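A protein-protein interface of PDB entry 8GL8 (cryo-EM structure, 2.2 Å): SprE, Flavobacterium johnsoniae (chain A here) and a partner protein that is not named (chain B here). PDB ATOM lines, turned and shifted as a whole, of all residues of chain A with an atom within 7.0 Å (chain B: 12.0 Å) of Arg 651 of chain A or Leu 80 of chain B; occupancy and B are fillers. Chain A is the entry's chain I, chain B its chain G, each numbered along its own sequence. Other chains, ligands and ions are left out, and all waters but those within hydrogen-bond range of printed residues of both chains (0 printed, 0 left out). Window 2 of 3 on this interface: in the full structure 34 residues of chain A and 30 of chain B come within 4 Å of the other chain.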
ATOM      1  N   LEU A 618      15.272 -11.886   7.212  1.00  0.00           N
ATOM      2  CA  LEU A 618      15.828 -10.881   8.110  1.00  0.00           C
ATOM      3  C   LEU A 618      17.268 -11.203   8.514  1.00  0.00           C
ATOM      4  O   LEU A 618      18.106 -10.291   8.543  1.00  0.00           O
ATOM      5  CB  LEU A 618      14.928 -10.722   9.337  1.00  0.00           C
ATOM      6  CG  LEU A 618      14.769  -9.294   9.858  1.00  0.00           C
ATOM      7  CD1 LEU A 618      13.816  -8.519   8.969  1.00  0.00           C
ATOM      8  CD2 LEU A 618      14.245  -9.312  11.276  1.00  0.00           C
ATOM      9  N   PRO A 619      17.609 -12.456   8.853  1.00  0.00           N
ATOM     10  CA  PRO A 619      19.034 -12.763   9.061  1.00  0.00           C
ATOM     11  C   PRO A 619      19.886 -12.534   7.823  1.00  0.00           C
ATOM     12  O   PRO A 619      21.034 -12.090   7.943  1.00  0.00           O
ATOM     13  CB  PRO A 619      19.021 -14.240   9.484  1.00  0.00           C
ATOM     14  CG  PRO A 619      17.701 -14.756   9.056  1.00  0.00           C
ATOM     15  CD  PRO A 619      16.765 -13.609   9.207  1.00  0.00           C
ATOM     16  N   TYR A 622      20.507  -8.850   7.687  1.00  0.00           N
ATOM     17  CA  TYR A 622      21.536  -8.449   8.644  1.00  0.00           C
ATOM     18  C   TYR A 622      22.931  -8.836   8.161  1.00  0.00           C
ATOM     19  O   TYR A 622      23.889  -8.064   8.314  1.00  0.00           O
ATOM     20  CB  TYR A 622      21.255  -9.069  10.010  1.00  0.00           C
ATOM     21  CG  TYR A 622      22.373  -8.866  11.003  1.00  0.00           C
ATOM     22  CD1 TYR A 622      22.699  -7.598  11.460  1.00  0.00           C
ATOM     23  CD2 TYR A 622      23.104  -9.942  11.483  1.00  0.00           C
ATOM     24  CE1 TYR A 622      23.720  -7.407  12.366  1.00  0.00           C
ATOM     25  CE2 TYR A 622      24.127  -9.761  12.390  1.00  0.00           C
ATOM     26  CZ  TYR A 622      24.431  -8.492  12.828  1.00  0.00           C
ATOM     27  OH  TYR A 622      25.450  -8.307  13.732  1.00  0.00           O
ATOM     28  N   ASN A 623      23.070 -10.032   7.588  1.00  0.00           N
ATOM     29  CA  ASN A 623      24.365 -10.446   7.059  1.00  0.00           C
ATOM     30  C   ASN A 623      24.788  -9.564   5.890  1.00  0.00           C
ATOM     31  O   ASN A 623      25.969  -9.222   5.758  1.00  0.00           O
ATOM     32  CB  ASN A 623      24.316 -11.914   6.643  1.00  0.00           C
ATOM     33  CG  ASN A 623      24.511 -12.851   7.814  1.00  0.00           C
ATOM     34  OD1 ASN A 623      25.546 -12.825   8.478  1.00  0.00           O
ATOM     35  ND2 ASN A 623      23.512 -13.683   8.078  1.00  0.00           N
ATOM     36  N   PRO A 648      10.866  -3.701  11.426  1.00  0.00           N
ATOM     37  CA  PRO A 648      11.536  -3.610  12.729  1.00  0.00           C
ATOM     38  C   PRO A 648      11.590  -4.958  13.429  1.00  0.00           C
ATOM     39  O   PRO A 648      10.579  -5.449  13.937  1.00  0.00           O
ATOM     40  CB  PRO A 648      10.676  -2.605  13.506  1.00  0.00           C
ATOM     41  CG  PRO A 648       9.342  -2.646  12.851  1.00  0.00           C
ATOM     42  CD  PRO A 648       9.547  -3.045  11.419  1.00  0.00           C
ATOM     43  N   GLY A 649      12.780  -5.559  13.462  1.00  0.00           N
ATOM     44  CA  GLY A 649      12.936  -6.880  14.028  1.00  0.00           C
ATOM     45  C   GLY A 649      12.906  -6.885  15.542  1.00  0.00           C
ATOM     46  O   GLY A 649      12.993  -5.851  16.205  1.00  0.00           O
ATOM     47  N   SER A 650      12.768  -8.093  16.093  1.00  0.00           N
ATOM     48  CA  SER A 650      12.767  -8.249  17.542  1.00  0.00           C
ATOM     49  C   SER A 650      14.105  -7.835  18.142  1.00  0.00           C
ATOM     50  O   SER A 650      14.148  -7.165  19.180  1.00  0.00           O
ATOM     51  CB  SER A 650      12.435  -9.695  17.914  1.00  0.00           C
ATOM     52  OG  SER A 650      11.068  -9.834  18.260  1.00  0.00           O
ATOM     53  N   ARG A 651      15.204  -8.219  17.500  1.00  0.00           N
ATOM     54  CA  ARG A 651      16.534  -7.887  17.993  1.00  0.00           C
ATOM     55  C   ARG A 651      17.313  -7.065  16.975  1.00  0.00           C
ATOM     56  O   ARG A 651      18.107  -6.196  17.349  1.00  0.00           O
ATOM     57  CB  ARG A 651      17.308  -9.161  18.339  1.00  0.00           C
ATOM     58  CG  ARG A 651      16.542 -10.160  19.188  1.00  0.00           C
ATOM     59  CD  ARG A 651      16.709  -9.858  20.669  1.00  0.00           C
ATOM     60  NE  ARG A 651      17.834  -8.964  20.917  1.00  0.00           N
ATOM     61  CZ  ARG A 651      18.099  -8.398  22.086  1.00  0.00           C
ATOM     62  NH1 ARG A 651      17.347  -8.623  23.149  1.00  0.00           N
ATOM     63  NH2 ARG A 651      19.150  -7.588  22.192  1.00  0.00           N
ATOM     64  N   TYR A 652      17.088  -7.330  15.687  1.00  0.00           N
ATOM     65  CA  TYR A 652      17.889  -6.700  14.644  1.00  0.00           C
ATOM     66  C   TYR A 652      17.710  -5.187  14.640  1.00  0.00           C
ATOM     67  O   TYR A 652      18.689  -4.434  14.576  1.00  0.00           O
ATOM     68  CB  TYR A 652      17.519  -7.290  13.282  1.00  0.00           C
ATOM     69  CG  TYR A 652      17.797  -8.770  13.162  1.00  0.00           C
ATOM     70  CD1 TYR A 652      19.041  -9.232  12.762  1.00  0.00           C
ATOM     71  CD2 TYR A 652      16.819  -9.705  13.465  1.00  0.00           C
ATOM     72  CE1 TYR A 652      19.298 -10.583  12.655  1.00  0.00           C
ATOM     73  CE2 TYR A 652      17.066 -11.057  13.360  1.00  0.00           C
ATOM     74  CZ  TYR A 652      18.308 -11.490  12.956  1.00  0.00           C
ATOM     75  OH  TYR A 652      18.560 -12.837  12.853  1.00  0.00           O
ATOM     76  N   ALA A 653      16.460  -4.723  14.723  1.00  0.00           N
ATOM     77  CA  ALA A 653      16.193  -3.293  14.615  1.00  0.00           C
ATOM     78  C   ALA A 653      16.844  -2.514  15.750  1.00  0.00           C
ATOM     79  O   ALA A 653      17.419  -1.443  15.526  1.00  0.00           O
ATOM     80  CB  ALA A 653      14.687  -3.042  14.589  1.00  0.00           C
ATOM     81  N   GLN A 654      16.772  -3.033  16.972  1.00  0.00           N
ATOM     82  CA  GLN A 654      17.299  -2.313  18.125  1.00  0.00           C
ATOM     83  C   GLN A 654      18.791  -2.531  18.341  1.00  0.00           C
ATOM     84  O   GLN A 654      19.360  -1.920  19.251  1.00  0.00           O
ATOM     85  CB  GLN A 654      16.526  -2.702  19.385  1.00  0.00           C
ATOM     86  CG  GLN A 654      15.978  -4.109  19.365  1.00  0.00           C
ATOM     87  CD  GLN A 654      14.837  -4.282  20.340  1.00  0.00           C
ATOM     88  OE1 GLN A 654      14.951  -3.934  21.515  1.00  0.00           O
ATOM     89  NE2 GLN A 654      13.721  -4.813  19.856  1.00  0.00           N
ATOM     90  N   ILE A 655      19.435  -3.375  17.538  1.00  0.00           N
ATOM     91  CA  ILE A 655      20.877  -3.571  17.630  1.00  0.00           C
ATOM     92  C   ILE A 655      21.548  -2.791  16.508  1.00  0.00           C
ATOM     93  O   ILE A 655      22.668  -2.291  16.669  1.00  0.00           O
ATOM     94  CB  ILE A 655      21.242  -5.067  17.587  1.00  0.00           C
ATOM     95  CG1 ILE A 655      20.805  -5.752  18.885  1.00  0.00           C
ATOM     96  CG2 ILE A 655      22.734  -5.261  17.363  1.00  0.00           C
ATOM     97  CD1 ILE A 655      21.549  -7.036  19.190  1.00  0.00           C
ATOM     98  N   LEU A 656      20.862  -2.655  15.369  1.00  0.00           N
ATOM     99  CA  LEU A 656      21.417  -1.865  14.274  1.00  0.00           C
ATOM    100  C   LEU A 656      21.626  -0.415  14.692  1.00  0.00           C
ATOM    101  O   LEU A 656      22.664   0.183  14.385  1.00  0.00           O
ATOM    102  CB  LEU A 656      20.517  -1.948  13.042  1.00  0.00           C
ATOM    103  CG  LEU A 656      20.502  -3.271  12.274  1.00  0.00           C
ATOM    104  CD1 LEU A 656      20.206  -3.032  10.805  1.00  0.00           C
ATOM    105  CD2 LEU A 656      21.820  -4.014  12.441  1.00  0.00           C
ATOM    106  N   ASN A 660      18.774  -0.458  23.083  1.00  0.00           N
ATOM    107  CA  ASN A 660      18.849  -0.953  24.454  1.00  0.00           C
ATOM    108  C   ASN A 660      18.576  -2.449  24.507  1.00  0.00           C
ATOM    109  O   ASN A 660      18.313  -3.079  23.478  1.00  0.00           O
ATOM    110  CB  ASN A 660      17.852  -0.215  25.354  1.00  0.00           C
ATOM    111  CG  ASN A 660      18.287  -0.187  26.807  1.00  0.00           C
ATOM    112  OD1 ASN A 660      19.300  -0.780  27.175  1.00  0.00           O
ATOM    113  ND2 ASN A 660      17.516   0.500  27.643  1.00  0.00           N
ATOM    114  N   THR A 661      18.639  -3.026  25.708  1.00  0.00           N
ATOM    115  CA  THR A 661      18.174  -4.383  25.962  1.00  0.00           C
ATOM    116  C   THR A 661      16.742  -4.398  26.485  1.00  0.00           C
ATOM    117  O   THR A 661      16.372  -5.279  27.269  1.00  0.00           O
ATOM    118  CB  THR A 661      19.105  -5.095  26.943  1.00  0.00           C
ATOM    119  OG1 THR A 661      19.164  -4.356  28.169  1.00  0.00           O
ATOM    120  CG2 THR A 661      20.505  -5.211  26.360  1.00  0.00           C
ATOM    121  N   ASP A 662      15.931  -3.421  26.067  1.00  0.00           N
ATOM    122  CA  ASP A 662      14.569  -3.302  26.577  1.00  0.00           C
ATOM    123  C   ASP A 662      13.717  -4.501  26.183  1.00  0.00           C
ATOM    124  O   ASP A 662      12.886  -4.965  26.973  1.00  0.00           O
ATOM    125  CB  ASP A 662      13.935  -2.005  26.072  1.00  0.00           C
ATOM    126  CG  ASP A 662      12.503  -1.836  26.540  1.00  0.00           C
ATOM    127  OD1 ASP A 662      12.193  -2.255  27.675  1.00  0.00           O
ATOM    128  OD2 ASP A 662      11.686  -1.284  25.773  1.00  0.00           O
ATOM    129  N   ASP A 663      13.894  -5.004  24.962  1.00  0.00           N
ATOM    130  CA  ASP A 663      13.143  -6.170  24.518  1.00  0.00           C
ATOM    131  C   ASP A 663      13.411  -7.354  25.437  1.00  0.00           C
ATOM    132  O   ASP A 663      14.561  -7.648  25.778  1.00  0.00           O
ATOM    133  CB  ASP A 663      13.506  -6.524  23.076  1.00  0.00           C
ATOM    134  CG  ASP A 663      15.004  -6.598  22.852  1.00  0.00           C
ATOM    135  OD1 ASP A 663      15.769  -6.224  23.766  1.00  0.00           O
ATOM    136  OD2 ASP A 663      15.418  -7.032  21.758  1.00  0.00           O
ATOM    137  N   ILE A 664      12.344  -8.032  25.839  1.00  0.00           N
ATOM    138  CA  ILE A 664      12.438  -9.080  26.850  1.00  0.00           C
ATOM    139  C   ILE A 664      12.991 -10.354  26.217  1.00  0.00           C
ATOM    140  O   ILE A 664      12.446 -10.845  25.216  1.00  0.00           O
ATOM    141  CB  ILE A 664      11.077  -9.299  27.537  1.00  0.00           C
ATOM    142  CG1 ILE A 664      11.226 -10.237  28.731  1.00  0.00           C
ATOM    143  CG2 ILE A 664      10.006  -9.779  26.553  1.00  0.00           C
ATOM    144  CD1 ILE A 664      12.099  -9.686  29.837  1.00  0.00           C
ATOM    145  N   PRO A 665      14.091 -10.894  26.732  1.00  0.00           N
ATOM    146  CA  PRO A 665      14.646 -12.135  26.186  1.00  0.00           C
ATOM    147  C   PRO A 665      14.028 -13.367  26.831  1.00  0.00           C
ATOM    148  O   PRO A 665      13.399 -13.307  27.889  1.00  0.00           O
ATOM    149  CB  PRO A 665      16.143 -12.037  26.530  1.00  0.00           C
ATOM    150  CG  PRO A 665      16.336 -10.684  27.194  1.00  0.00           C
ATOM    151  CD  PRO A 665      14.998 -10.284  27.713  1.00  0.00           C
ATOM    152  N   GLU B  72      34.395  -7.883  23.071  1.00  0.00           N
ATOM    153  CA  GLU B  72      33.346  -6.871  23.014  1.00  0.00           C
ATOM    154  C   GLU B  72      32.489  -7.034  21.767  1.00  0.00           C
ATOM    155  O   GLU B  72      31.263  -6.884  21.823  1.00  0.00           O
ATOM    156  CB  GLU B  72      33.960  -5.473  23.065  1.00  0.00           C
ATOM    157  CG  GLU B  72      32.940  -4.356  23.182  1.00  0.00           C
ATOM    158  CD  GLU B  72      31.966  -4.575  24.322  1.00  0.00           C
ATOM    159  OE1 GLU B  72      32.422  -4.866  25.447  1.00  0.00           O
ATOM    160  OE2 GLU B  72      30.744  -4.456  24.093  1.00  0.00           O
ATOM    161  N   GLY B  73      33.116  -7.338  20.629  1.00  0.00           N
ATOM    162  CA  GLY B  73      32.351  -7.565  19.416  1.00  0.00           C
ATOM    163  C   GLY B  73      31.415  -8.751  19.533  1.00  0.00           C
ATOM    164  O   GLY B  73      30.273  -8.700  19.070  1.00  0.00           O
ATOM    165  N   LEU B  74      31.886  -9.838  20.149  1.00  0.00           N
ATOM    166  CA  LEU B  74      31.016 -10.990  20.359  1.00  0.00           C
ATOM    167  C   LEU B  74      29.869 -10.636  21.296  1.00  0.00           C
ATOM    168  O   LEU B  74      28.716 -11.009  21.049  1.00  0.00           O
ATOM    169  CB  LEU B  74      31.824 -12.166  20.913  1.00  0.00           C
ATOM    170  CG  LEU B  74      31.125 -13.337  21.619  1.00  0.00           C
ATOM    171  CD1 LEU B  74      29.945 -13.879  20.818  1.00  0.00           C
ATOM    172  CD2 LEU B  74      32.112 -14.450  21.925  1.00  0.00           C
ATOM    173  N   LYS B  75      30.162  -9.903  22.373  1.00  0.00           N
ATOM    174  CA  LYS B  75      29.127  -9.558  23.341  1.00  0.00           C
ATOM    175  C   LYS B  75      28.061  -8.658  22.726  1.00  0.00           C
ATOM    176  O   LYS B  75      26.871  -8.807  23.024  1.00  0.00           O
ATOM    177  CB  LYS B  75      29.757  -8.886  24.560  1.00  0.00           C
ATOM    178  CG  LYS B  75      28.758  -8.455  25.618  1.00  0.00           C
ATOM    179  CD  LYS B  75      29.393  -7.515  26.629  1.00  0.00           C
ATOM    180  CE  LYS B  75      28.347  -6.654  27.319  1.00  0.00           C
ATOM    181  NZ  LYS B  75      26.998  -7.283  27.281  1.00  0.00           N
ATOM    182  N   THR B  76      28.469  -7.718  21.871  1.00  0.00           N
ATOM    183  CA  THR B  76      27.526  -6.743  21.330  1.00  0.00           C
ATOM    184  C   THR B  76      26.440  -7.418  20.496  1.00  0.00           C
ATOM    185  O   THR B  76      25.251  -7.112  20.641  1.00  0.00           O
ATOM    186  CB  THR B  76      28.277  -5.700  20.499  1.00  0.00           C
ATOM    187  OG1 THR B  76      28.838  -4.709  21.368  1.00  0.00           O
ATOM    188  CG2 THR B  76      27.343  -5.022  19.508  1.00  0.00           C
ATOM    189  N   GLU B  77      26.826  -8.351  19.631  1.00  0.00           N
ATOM    190  CA  GLU B  77      25.905  -8.995  18.700  1.00  0.00           C
ATOM    191  C   GLU B  77      25.715 -10.474  19.022  1.00  0.00           C
ATOM    192  O   GLU B  77      25.563 -11.306  18.126  1.00  0.00           O
ATOM    193  CB  GLU B  77      26.385  -8.824  17.263  1.00  0.00           C
ATOM    194  CG  GLU B  77      27.808  -9.299  17.029  1.00  0.00           C
ATOM    195  CD  GLU B  77      28.258  -9.108  15.596  1.00  0.00           C
ATOM    196  OE1 GLU B  77      27.434  -9.310  14.680  1.00  0.00           O
ATOM    197  OE2 GLU B  77      29.438  -8.757  15.385  1.00  0.00           O
ATOM    198  N   LYS B  78      25.717 -10.819  20.310  1.00  0.00           N
ATOM    199  CA  LYS B  78      25.570 -12.214  20.701  1.00  0.00           C
ATOM    200  C   LYS B  78      24.159 -12.738  20.466  1.00  0.00           C
ATOM    201  O   LYS B  78      23.982 -13.949  20.300  1.00  0.00           O
ATOM    202  CB  LYS B  78      25.954 -12.390  22.170  1.00  0.00           C
ATOM    203  CG  LYS B  78      26.348 -13.805  22.533  1.00  0.00           C
ATOM    204  CD  LYS B  78      26.987 -13.880  23.906  1.00  0.00           C
ATOM    205  CE  LYS B  78      27.159 -15.324  24.345  1.00  0.00           C
ATOM    206  NZ  LYS B  78      28.555 -15.611  24.778  1.00  0.00           N
ATOM    207  N   ALA B  79      23.156 -11.859  20.447  1.00  0.00           N
ATOM    208  CA  ALA B  79      21.778 -12.300  20.262  1.00  0.00           C
ATOM    209  C   ALA B  79      21.470 -12.657  18.814  1.00  0.00           C
ATOM    210  O   ALA B  79      20.626 -13.525  18.563  1.00  0.00           O
ATOM    211  CB  ALA B  79      20.813 -11.218  20.747  1.00  0.00           C
ATOM    212  N   LEU B  80      22.131 -12.012  17.858  1.00  0.00           N
ATOM    213  CA  LEU B  80      21.842 -12.203  16.443  1.00  0.00           C
ATOM    214  C   LEU B  80      22.568 -13.394  15.835  1.00  0.00           C
ATOM    215  O   LEU B  80      22.377 -13.674  14.648  1.00  0.00           O
ATOM    216  CB  LEU B  80      22.200 -10.936  15.662  1.00  0.00           C
ATOM    217  CG  LEU B  80      21.446  -9.676  16.083  1.00  0.00           C
ATOM    218  CD1 LEU B  80      21.738  -8.531  15.134  1.00  0.00           C
ATOM    219  CD2 LEU B  80      19.963  -9.962  16.132  1.00  0.00           C
ATOM    220  N   LEU B  81      23.389 -14.096  16.605  1.00  0.00           N
ATOM    221  CA  LEU B  81      24.160 -15.219  16.096  1.00  0.00           C
ATOM    222  C   LEU B  81      23.514 -16.539  16.497  1.00  0.00           C
ATOM    223  O   LEU B  81      22.869 -16.646  17.542  1.00  0.00           O
ATOM    224  CB  LEU B  81      25.599 -15.172  16.613  1.00  0.00           C
ATOM    225  CG  LEU B  81      26.418 -13.924  16.288  1.00  0.00           C
ATOM    226  CD1 LEU B  81      27.889 -14.174  16.559  1.00  0.00           C
ATOM    227  CD2 LEU B  81      26.204 -13.497  14.846  1.00  0.00           C
ATOM    228  N   THR B  82      23.694 -17.545  15.648  1.00  0.00           N
ATOM    229  CA  THR B  82      23.258 -18.892  15.971  1.00  0.00           C
ATOM    230  C   THR B  82      24.238 -19.538  16.947  1.00  0.00           C
ATOM    231  O   THR B  82      25.310 -19.005  17.236  1.00  0.00           O
ATOM    232  CB  THR B  82      23.134 -19.739  14.706  1.00  0.00           C
ATOM    233  OG1 THR B  82      23.414 -21.109  15.018  1.00  0.00           O
ATOM    234  CG2 THR B  82      24.113 -19.258  13.647  1.00  0.00           C
ATOM    235  N   LYS B  83      23.854 -20.708  17.461  1.00  0.00           N
ATOM    236  CA  LYS B  83      24.712 -21.407  18.413  1.00  0.00           C
ATOM    237  C   LYS B  83      26.043 -21.790  17.779  1.00  0.00           C
ATOM    238  O   LYS B  83      27.098 -21.679  18.418  1.00  0.00           O
ATOM    239  CB  LYS B  83      23.999 -22.644  18.956  1.00  0.00           C
ATOM    240  CG  LYS B  83      23.972 -22.721  20.473  1.00  0.00           C
ATOM    241  CD  LYS B  83      23.486 -24.079  20.954  1.00  0.00           C
ATOM    242  CE  LYS B  83      23.435 -24.142  22.472  1.00  0.00           C
ATOM    243  NZ  LYS B  83      22.802 -25.399  22.959  1.00  0.00           N
ATOM    244  N   GLU B  84      26.016 -22.240  16.522  1.00  0.00           N
ATOM    245  CA  GLU B  84      27.250 -22.627  15.846  1.00  0.00           C
ATOM    246  C   GLU B  84      28.197 -21.442  15.708  1.00  0.00           C
ATOM    247  O   GLU B  84      29.390 -21.547  16.020  1.00  0.00           O
ATOM    248  CB  GLU B  84      26.930 -23.222  14.476  1.00  0.00           C
ATOM    249  CG  GLU B  84      26.154 -24.525  14.530  1.00  0.00           C
ATOM    250  CD  GLU B  84      24.705 -24.353  14.121  1.00  0.00           C
ATOM    251  OE1 GLU B  84      24.131 -23.280  14.403  1.00  0.00           O
ATOM    252  OE2 GLU B  84      24.141 -25.289  13.516  1.00  0.00           O
ATOM    253  N   LEU B  85      27.681 -20.301  15.244  1.00  0.00           N
ATOM    254  CA  LEU B  85      28.524 -19.124  15.069  1.00  0.00           C
ATOM    255  C   LEU B  85      29.085 -18.643  16.400  1.00  0.00           C
ATOM    256  O   LEU B  85      30.255 -18.252  16.485  1.00  0.00           O
ATOM    257  CB  LEU B  85      27.734 -18.008  14.386  1.00  0.00           C
ATOM    258  CG  LEU B  85      27.770 -17.984  12.858  1.00  0.00           C
ATOM    259  CD1 LEU B  85      27.356 -16.618  12.336  1.00  0.00           C
ATOM    260  CD2 LEU B  85      29.150 -18.358  12.346  1.00  0.00           C
ATOM    261  N   ILE B  86      28.259 -18.659  17.448  1.00  0.00           N
ATOM    262  CA  ILE B  86      28.738 -18.305  18.780  1.00  0.00           C
ATOM    263  C   ILE B  86      29.871 -19.232  19.194  1.00  0.00           C
ATOM    264  O   ILE B  86      30.874 -18.794  19.771  1.00  0.00           O
ATOM    265  CB  ILE B  86      27.578 -18.346  19.791  1.00  0.00           C
ATOM    266  CG1 ILE B  86      26.568 -17.239  19.489  1.00  0.00           C
ATOM    267  CG2 ILE B  86      28.106 -18.230  21.213  1.00  0.00           C
ATOM    268  CD1 ILE B  86      25.792 -16.767  20.693  1.00  0.00           C
ATOM    269  N   GLU B  87      29.733 -20.526  18.898  1.00  0.00           N
ATOM    270  CA  GLU B  87      30.786 -21.476  19.240  1.00  0.00           C
ATOM    271  C   GLU B  87      32.081 -21.161  18.502  1.00  0.00           C
ATOM    272  O   GLU B  87      33.162 -21.202  19.097  1.00  0.00           O
ATOM    273  CB  GLU B  87      30.324 -22.900  18.936  1.00  0.00           C
ATOM    274  CG  GLU B  87      30.008 -23.724  20.173  1.00  0.00           C
ATOM    275  CD  GLU B  87      29.058 -24.868  19.885  1.00  0.00           C
ATOM    276  OE1 GLU B  87      29.190 -25.498  18.816  1.00  0.00           O
ATOM    277  OE2 GLU B  87      28.177 -25.137  20.729  1.00  0.00           O
ATOM    278  N   ARG B  89      33.078 -18.223  17.291  1.00  0.00           N
ATOM    279  CA  ARG B  89      33.659 -16.993  17.827  1.00  0.00           C
ATOM    280  C   ARG B  89      34.309 -17.235  19.183  1.00  0.00           C
ATOM    281  O   ARG B  89      35.399 -16.718  19.460  1.00  0.00           O
ATOM    282  CB  ARG B  89      32.596 -15.899  17.927  1.00  0.00           C
ATOM    283  CG  ARG B  89      31.818 -15.672  16.646  1.00  0.00           C
ATOM    284  CD  ARG B  89      32.473 -14.630  15.764  1.00  0.00           C
ATOM    285  NE  ARG B  89      32.101 -13.276  16.153  1.00  0.00           N
ATOM    286  CZ  ARG B  89      31.430 -12.435  15.376  1.00  0.00           C
ATOM    287  NH1 ARG B  89      31.039 -12.780  14.162  1.00  0.00           N
ATOM    288  NH2 ARG B  89      31.147 -11.218  15.831  1.00  0.00           N
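Printed residues of chain A that touch a printed residue of chain B: Tyr 622, Arg 651, Tyr 652 and Ile 655. Hydrophobic or aromatic side chains of chain A that line the printed part of chain B: Tyr 622, Tyr 652 and Ile 655. Among the printed residues, no Asp or Glu carboxylate lies within 4 Å of a Lys or Arg side-chain nitrogen of the other chain.
Of chain B, only Ala 79 (3.7 Å) and Leu 80 (3.5 Å) come within 4 Å of Arg 651 of chain A. Leu 80 of chain B touches three residues of chain A. No residue of chain B comes within 4 Å of Pro 619 of chain A. Tyr 622 of chain A touches just these residues of chain B: Glu 77 and Leu 80. No residue of chain B comes within 4 Å of Gly 649 of chain A. Ser 650 of chain A touches none of the printed residues of chain B. Tyr 652 of chain A touches just one residue of chain B: Leu 80 (3.6 Å). No residue of chain B comes within 4 Å of Ala 653 of chain A. No residue of chain B comes within 4 Å of Gln 654 of chain A. Ile 655 of chain A touches just one residue of chain B: Thr 76 (3.98 Å). No residue of chain B comes within 4 Å of Thr 661 of chain A. No residue of chain B comes within 4 Å of Asp 663 of chain A. Of the printed residues of chain A, Ala 79 of chain B touches Arg 651 (3.7 Å). Of the printed residues of chain A, Thr 76 of chain B touches Ile 655. Of the printed residues of chain A, Glu 77 of chain B touches Tyr 622.
OH of Tyr 622 of chain A lies within hydrogen-bond range of OE1 of Glu 77 of chain B, at 2.4 Å.
Among the printed residues, merely in contact across the chains: Arg 651 of chain A with Leu 80 of chain B (3.5 Å), Tyr 622 of chain A with Leu 80 of chain B (3.5 Å), Tyr 652 of chain A with Leu 80 of chain B (3.6 Å), Arg 651 of chain A with Ala 79 of chain B (3.7 Å) and Ile 655 of chain A with Thr 76 of chain B (3.98 Å).
O of Glu 72 of chain B sits at hydrogen-bond distance from OG1 of Thr 76 of chain B (3.3 Å). The side-chain carboxylate (OE2) of Glu 77 of chain B is in salt-bridge range of the guanidinium group (NH2) of Arg 89 of chain B (3.0 Å). The guanidinium group of Arg 651 of chain A lies within salt-bridge range of the side-chain carboxylate of Asp 663 of chain A, 2.9 Å away.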
